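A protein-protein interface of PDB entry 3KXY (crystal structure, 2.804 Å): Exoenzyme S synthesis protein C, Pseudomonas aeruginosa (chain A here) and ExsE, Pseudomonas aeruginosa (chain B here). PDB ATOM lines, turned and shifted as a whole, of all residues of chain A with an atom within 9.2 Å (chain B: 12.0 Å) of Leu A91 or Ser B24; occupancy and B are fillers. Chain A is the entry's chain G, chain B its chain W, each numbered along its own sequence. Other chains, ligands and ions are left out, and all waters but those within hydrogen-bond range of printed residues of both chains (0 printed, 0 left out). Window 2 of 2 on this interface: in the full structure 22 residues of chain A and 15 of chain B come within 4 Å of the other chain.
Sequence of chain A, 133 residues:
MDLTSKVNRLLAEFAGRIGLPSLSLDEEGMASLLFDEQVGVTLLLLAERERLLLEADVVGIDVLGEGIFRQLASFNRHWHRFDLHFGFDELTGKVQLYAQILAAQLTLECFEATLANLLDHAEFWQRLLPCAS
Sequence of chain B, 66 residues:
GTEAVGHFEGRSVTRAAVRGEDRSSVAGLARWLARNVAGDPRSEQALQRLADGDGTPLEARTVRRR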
ATOM      1  N   MET A  30      34.833 -17.530 -37.769  1.00  0.00           N
ATOM      2  CA  MET A  30      34.760 -17.197 -36.352  1.00  0.00           C
ATOM      3  C   MET A  30      35.482 -18.227 -35.488  1.00  0.00           C
ATOM      4  O   MET A  30      35.614 -19.390 -35.866  1.00  0.00           O
ATOM      5  CB  MET A  30      33.298 -17.074 -35.905  1.00  0.00           C
ATOM      6  CG  MET A  30      32.511 -15.999 -36.640  1.00  0.00           C
ATOM      7  SD  MET A  30      30.776 -15.937 -36.151  1.00  0.00           S
ATOM      8  CE  MET A  30      30.917 -15.554 -34.407  1.00  0.00           C
ATOM      9  N   GLU A  55      35.664  -9.591 -30.093  1.00  0.00           N
ATOM     10  CA  GLU A  55      34.621  -9.361 -29.102  1.00  0.00           C
ATOM     11  C   GLU A  55      35.047  -9.910 -27.745  1.00  0.00           C
ATOM     12  O   GLU A  55      35.699 -10.951 -27.664  1.00  0.00           O
ATOM     13  CB  GLU A  55      33.304 -10.005 -29.539  1.00  0.00           C
ATOM     14  CG  GLU A  55      32.690  -9.389 -30.786  1.00  0.00           C
ATOM     15  CD  GLU A  55      31.368 -10.031 -31.160  1.00  0.00           C
ATOM     16  OE1 GLU A  55      30.957 -10.994 -30.477  1.00  0.00           O
ATOM     17  OE2 GLU A  55      30.739  -9.573 -32.138  1.00  0.00           O
ATOM     18  N   ILE A  61      24.234  -8.067 -17.302  1.00  0.00           N
ATOM     19  CA  ILE A  61      23.391  -6.922 -16.979  1.00  0.00           C
ATOM     20  C   ILE A  61      22.657  -7.104 -15.651  1.00  0.00           C
ATOM     21  O   ILE A  61      22.213  -6.133 -15.038  1.00  0.00           O
ATOM     22  CB  ILE A  61      22.367  -6.650 -18.101  1.00  0.00           C
ATOM     23  CG1 ILE A  61      21.697  -5.288 -17.901  1.00  0.00           C
ATOM     24  CG2 ILE A  61      21.335  -7.769 -18.168  1.00  0.00           C
ATOM     25  CD1 ILE A  61      20.683  -4.946 -18.969  1.00  0.00           C
ATOM     26  N   PHE A  88      26.573  -3.986 -26.556  1.00  0.00           N
ATOM     27  CA  PHE A  88      25.694  -4.845 -25.770  1.00  0.00           C
ATOM     28  C   PHE A  88      25.008  -5.912 -26.617  1.00  0.00           C
ATOM     29  O   PHE A  88      24.605  -5.661 -27.753  1.00  0.00           O
ATOM     30  CB  PHE A  88      24.652  -4.007 -25.025  1.00  0.00           C
ATOM     31  CG  PHE A  88      23.770  -4.808 -24.112  1.00  0.00           C
ATOM     32  CD1 PHE A  88      24.229  -5.227 -22.875  1.00  0.00           C
ATOM     33  CD2 PHE A  88      22.477  -5.136 -24.487  1.00  0.00           C
ATOM     34  CE1 PHE A  88      23.420  -5.964 -22.031  1.00  0.00           C
ATOM     35  CE2 PHE A  88      21.663  -5.872 -23.647  1.00  0.00           C
ATOM     36  CZ  PHE A  88      22.135  -6.286 -22.417  1.00  0.00           C
ATOM     37  N   ASP A  89      24.883  -7.107 -26.051  1.00  0.00           N
ATOM     38  CA  ASP A  89      24.226  -8.216 -26.727  1.00  0.00           C
ATOM     39  C   ASP A  89      22.965  -8.599 -25.962  1.00  0.00           C
ATOM     40  O   ASP A  89      23.029  -9.322 -24.970  1.00  0.00           O
ATOM     41  CB  ASP A  89      25.173  -9.412 -26.825  1.00  0.00           C
ATOM     42  CG  ASP A  89      24.637 -10.512 -27.720  1.00  0.00           C
ATOM     43  OD1 ASP A  89      23.457 -10.437 -28.121  1.00  0.00           O
ATOM     44  OD2 ASP A  89      25.401 -11.454 -28.023  1.00  0.00           O
ATOM     45  N   GLU A  90      21.821  -8.109 -26.430  1.00  0.00           N
ATOM     46  CA  GLU A  90      20.550  -8.319 -25.743  1.00  0.00           C
ATOM     47  C   GLU A  90      20.259  -9.794 -25.482  1.00  0.00           C
ATOM     48  O   GLU A  90      19.672 -10.147 -24.458  1.00  0.00           O
ATOM     49  CB  GLU A  90      19.402  -7.690 -26.538  1.00  0.00           C
ATOM     50  CG  GLU A  90      18.041  -7.823 -25.873  1.00  0.00           C
ATOM     51  CD  GLU A  90      16.919  -7.240 -26.711  1.00  0.00           C
ATOM     52  OE1 GLU A  90      15.749  -7.327 -26.284  1.00  0.00           O
ATOM     53  OE2 GLU A  90      17.208  -6.695 -27.798  1.00  0.00           O
ATOM     54  N   LEU A  91      20.673 -10.651 -26.408  1.00  0.00           N
ATOM     55  CA  LEU A  91      20.393 -12.080 -26.309  1.00  0.00           C
ATOM     56  C   LEU A  91      21.162 -12.752 -25.175  1.00  0.00           C
ATOM     57  O   LEU A  91      20.664 -13.685 -24.548  1.00  0.00           O
ATOM     58  CB  LEU A  91      20.687 -12.787 -27.637  1.00  0.00           C
ATOM     59  CG  LEU A  91      19.740 -12.523 -28.812  1.00  0.00           C
ATOM     60  CD1 LEU A  91      19.849 -11.085 -29.303  1.00  0.00           C
ATOM     61  CD2 LEU A  91      20.017 -13.495 -29.948  1.00  0.00           C
ATOM     62  N   THR A  92      22.375 -12.273 -24.915  1.00  0.00           N
ATOM     63  CA  THR A  92      23.227 -12.870 -23.893  1.00  0.00           C
ATOM     64  C   THR A  92      23.161 -12.099 -22.581  1.00  0.00           C
ATOM     65  O   THR A  92      23.356 -12.666 -21.507  1.00  0.00           O
ATOM     66  CB  THR A  92      24.698 -12.931 -24.348  1.00  0.00           C
ATOM     67  OG1 THR A  92      24.764 -13.349 -25.716  1.00  0.00           O
ATOM     68  CG2 THR A  92      25.485 -13.904 -23.482  1.00  0.00           C
ATOM     69  N   GLY A  93      22.884 -10.802 -22.676  1.00  0.00           N
ATOM     70  CA  GLY A  93      22.869  -9.939 -21.509  1.00  0.00           C
ATOM     71  C   GLY A  93      24.279  -9.584 -21.078  1.00  0.00           C
ATOM     72  O   GLY A  93      24.522  -9.261 -19.915  1.00  0.00           O
ATOM     73  N   LYS A  94      25.209  -9.649 -22.024  1.00  0.00           N
ATOM     74  CA  LYS A  94      26.614  -9.380 -21.745  1.00  0.00           C
ATOM     75  C   LYS A  94      27.067  -8.047 -22.330  1.00  0.00           C
ATOM     76  O   LYS A  94      26.759  -7.724 -23.476  1.00  0.00           O
ATOM     77  CB  LYS A  94      27.491 -10.506 -22.299  1.00  0.00           C
ATOM     78  CG  LYS A  94      27.433 -11.801 -21.508  1.00  0.00           C
ATOM     79  CD  LYS A  94      28.130 -11.659 -20.165  1.00  0.00           C
ATOM     80  CE  LYS A  94      28.191 -12.986 -19.427  1.00  0.00           C
ATOM     81  NZ  LYS A  94      28.942 -12.869 -18.147  1.00  0.00           N
ATOM     82  N   GLN A  96      30.037  -5.870 -23.846  1.00  0.00           N
ATOM     83  CA  GLN A  96      31.186  -6.287 -24.645  1.00  0.00           C
ATOM     84  C   GLN A  96      32.107  -5.137 -25.046  1.00  0.00           C
ATOM     85  O   GLN A  96      31.649  -4.039 -25.362  1.00  0.00           O
ATOM     86  CB  GLN A  96      30.715  -7.026 -25.899  1.00  0.00           C
ATOM     87  CG  GLN A  96      29.926  -8.292 -25.617  1.00  0.00           C
ATOM     88  CD  GLN A  96      29.326  -8.891 -26.871  1.00  0.00           C
ATOM     89  OE1 GLN A  96      29.184  -8.212 -27.887  1.00  0.00           O
ATOM     90  NE2 GLN A  96      28.966 -10.167 -26.806  1.00  0.00           N
ATOM     91  N   TYR A  98      34.982  -4.021 -27.885  1.00  0.00           N
ATOM     92  CA  TYR A  98      35.358  -4.380 -29.245  1.00  0.00           C
ATOM     93  C   TYR A  98      36.700  -3.776 -29.646  1.00  0.00           C
ATOM     94  O   TYR A  98      36.974  -2.606 -29.382  1.00  0.00           O
ATOM     95  CB  TYR A  98      34.272  -3.961 -30.238  1.00  0.00           C
ATOM     96  CG  TYR A  98      32.883  -4.410 -29.850  1.00  0.00           C
ATOM     97  CD1 TYR A  98      32.547  -5.758 -29.825  1.00  0.00           C
ATOM     98  CD2 TYR A  98      31.904  -3.486 -29.513  1.00  0.00           C
ATOM     99  CE1 TYR A  98      31.277  -6.171 -29.469  1.00  0.00           C
ATOM    100  CE2 TYR A  98      30.632  -3.889 -29.158  1.00  0.00           C
ATOM    101  CZ  TYR A  98      30.324  -5.232 -29.136  1.00  0.00           C
ATOM    102  OH  TYR A  98      29.057  -5.630 -28.780  1.00  0.00           O
ATOM    103  N   ALA B  17      32.988 -22.829 -27.843  1.00  0.00           N
ATOM    104  CA  ALA B  17      32.092 -22.953 -28.986  1.00  0.00           C
ATOM    105  C   ALA B  17      31.659 -21.578 -29.482  1.00  0.00           C
ATOM    106  O   ALA B  17      31.473 -20.652 -28.692  1.00  0.00           O
ATOM    107  CB  ALA B  17      30.879 -23.798 -28.626  1.00  0.00           C
ATOM    108  N   VAL B  18      31.501 -21.452 -30.795  1.00  0.00           N
ATOM    109  CA  VAL B  18      31.125 -20.181 -31.401  1.00  0.00           C
ATOM    110  C   VAL B  18      29.680 -19.818 -31.066  1.00  0.00           C
ATOM    111  O   VAL B  18      29.305 -18.646 -31.087  1.00  0.00           O
ATOM    112  CB  VAL B  18      31.329 -20.212 -32.928  1.00  0.00           C
ATOM    113  CG1 VAL B  18      30.877 -18.905 -33.559  1.00  0.00           C
ATOM    114  CG2 VAL B  18      32.790 -20.485 -33.252  1.00  0.00           C
ATOM    115  N   ARG B  19      28.882 -20.833 -30.744  1.00  0.00           N
ATOM    116  CA  ARG B  19      27.480 -20.652 -30.363  1.00  0.00           C
ATOM    117  C   ARG B  19      26.744 -19.599 -31.196  1.00  0.00           C
ATOM    118  O   ARG B  19      25.989 -18.786 -30.663  1.00  0.00           O
ATOM    119  CB  ARG B  19      27.351 -20.360 -28.859  1.00  0.00           C
ATOM    120  CG  ARG B  19      28.244 -19.241 -28.320  1.00  0.00           C
ATOM    121  CD  ARG B  19      27.607 -17.869 -28.487  1.00  0.00           C
ATOM    122  NE  ARG B  19      28.397 -16.810 -27.866  1.00  0.00           N
ATOM    123  CZ  ARG B  19      29.281 -16.055 -28.512  1.00  0.00           C
ATOM    124  NH1 ARG B  19      29.490 -16.236 -29.808  1.00  0.00           N
ATOM    125  NH2 ARG B  19      29.953 -15.115 -27.861  1.00  0.00           N
ATOM    126  N   GLY B  20      26.960 -19.632 -32.508  1.00  0.00           N
ATOM    127  CA  GLY B  20      26.340 -18.677 -33.410  1.00  0.00           C
ATOM    128  C   GLY B  20      24.823 -18.697 -33.359  1.00  0.00           C
ATOM    129  O   GLY B  20      24.174 -17.671 -33.565  1.00  0.00           O
ATOM    130  N   GLU B  21      24.256 -19.868 -33.087  1.00  0.00           N
ATOM    131  CA  GLU B  21      22.807 -20.020 -33.019  1.00  0.00           C
ATOM    132  C   GLU B  21      22.294 -19.776 -31.604  1.00  0.00           C
ATOM    133  O   GLU B  21      21.106 -19.525 -31.397  1.00  0.00           O
ATOM    134  CB  GLU B  21      22.387 -21.415 -33.493  1.00  0.00           C
ATOM    135  CG  GLU B  21      22.639 -22.527 -32.481  1.00  0.00           C
ATOM    136  CD  GLU B  21      24.115 -22.798 -32.252  1.00  0.00           C
ATOM    137  OE1 GLU B  21      24.921 -22.531 -33.168  1.00  0.00           O
ATOM    138  OE2 GLU B  21      24.466 -23.287 -31.159  1.00  0.00           O
ATOM    139  N   ASP B  22      23.198 -19.854 -30.634  1.00  0.00           N
ATOM    140  CA  ASP B  22      22.841 -19.665 -29.233  1.00  0.00           C
ATOM    141  C   ASP B  22      22.595 -18.192 -28.919  1.00  0.00           C
ATOM    142  O   ASP B  22      21.560 -17.833 -28.357  1.00  0.00           O
ATOM    143  CB  ASP B  22      23.942 -20.217 -28.325  1.00  0.00           C
ATOM    144  CG  ASP B  22      23.568 -20.170 -26.857  1.00  0.00           C
ATOM    145  OD1 ASP B  22      24.481 -20.066 -26.011  1.00  0.00           O
ATOM    146  OD2 ASP B  22      22.360 -20.238 -26.548  1.00  0.00           O
ATOM    147  N   ARG B  23      23.550 -17.344 -29.289  1.00  0.00           N
ATOM    148  CA  ARG B  23      23.457 -15.915 -29.010  1.00  0.00           C
ATOM    149  C   ARG B  23      23.887 -15.079 -30.214  1.00  0.00           C
ATOM    150  O   ARG B  23      24.626 -15.552 -31.077  1.00  0.00           O
ATOM    151  CB  ARG B  23      24.315 -15.557 -27.794  1.00  0.00           C
ATOM    152  CG  ARG B  23      23.892 -16.243 -26.501  1.00  0.00           C
ATOM    153  CD  ARG B  23      22.520 -15.771 -26.044  1.00  0.00           C
ATOM    154  NE  ARG B  23      22.165 -16.292 -24.726  1.00  0.00           N
ATOM    155  CZ  ARG B  23      21.411 -17.368 -24.524  1.00  0.00           C
ATOM    156  NH1 ARG B  23      20.923 -18.044 -25.556  1.00  0.00           N
ATOM    157  NH2 ARG B  23      21.141 -17.769 -23.288  1.00  0.00           N
ATOM    158  N   SER B  24      23.419 -13.836 -30.263  1.00  0.00           N
ATOM    159  CA  SER B  24      23.773 -12.922 -31.345  1.00  0.00           C
ATOM    160  C   SER B  24      23.879 -11.485 -30.846  1.00  0.00           C
ATOM    161  O   SER B  24      22.993 -10.665 -31.089  1.00  0.00           O
ATOM    162  CB  SER B  24      22.751 -13.006 -32.481  1.00  0.00           C
ATOM    163  OG  SER B  24      23.067 -12.095 -33.520  1.00  0.00           O
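Of the printed residues of chain B, Met A30 touches Val B18 (3.5 Å). Of chain B, only Ser B24 (2.9 Å) comes within 4 Å of Asp A89. No residue of chain B comes within 4 Å of Glu A90. Of chain B, only Arg B23 (3.0 Å) and Ser B24 (3.4 Å) come within 4 Å of Leu A91. Of the printed residues of chain B, Thr A92 touches Arg B23. No residue of chain B comes within 4 Å of Gly A93. Tyr A98 touches none of the printed residues of chain B. Of the printed residues of chain A, Val B18 touches Met A30 (3.5 Å). Glu B21 touches none of the printed residues of chain A. Of chain A, only Leu A91 and Thr A92 come within 4 Å of Arg B23. Of chain A, only Asp A89 (2.9 Å) and Leu A91 (3.4 Å) come within 4 Å of Ser B24. The nearest printed residue of chain B that does not touch Met A30 is Arg B19 (4.9 Å).
Printed residues of chain B that touch a printed residue of chain A: Val B18, Arg B23 and Ser B24. Printed residues of chain A that touch a printed residue of chain B: Met A30, Asp A89, Leu A91 and Thr A92. Hydrophobic or aromatic side chains of chain A that line the printed part of chain B: Met A30 and Leu A91. Among the printed residues, 5 pairs touch across the chains. Among the printed residues, no Asp or Glu carboxylate lies within 4 Å of a Lys or Arg side-chain nitrogen of the other chain.
Among the printed residues, merely in contact across the chains: Met A30 with Val B18 (3.5 Å), Leu A91 with Ser B24 (3.4 Å) and Thr A92 with Arg B23 (3.1 Å).
The backbone carbonyl oxygen (O) of Leu A91 is in hydrogen-bond range of the guanidinium group (NE) of Arg B23 (3.0 Å). The side-chain carboxylate of Asp A89 lies close to the backbone carbonyl oxygen of Ser B24, 3.0 Å away.
The side-chain carboxylate of Asp A89 sits close to the backbone NH of Leu A91 (3.3 Å). OG1 of Thr A92 sits at hydrogen-bond distance from OD2 of Asp A89. The backbone NH (N) of Asp A89 lies within hydrogen-bond range of the backbone carbonyl oxygen (O) of Lys A94, at 3.2 Å. The guanidinium group of Arg B23 lies within salt-bridge range of the side-chain carboxylate of Asp B22 (2.8 Å).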
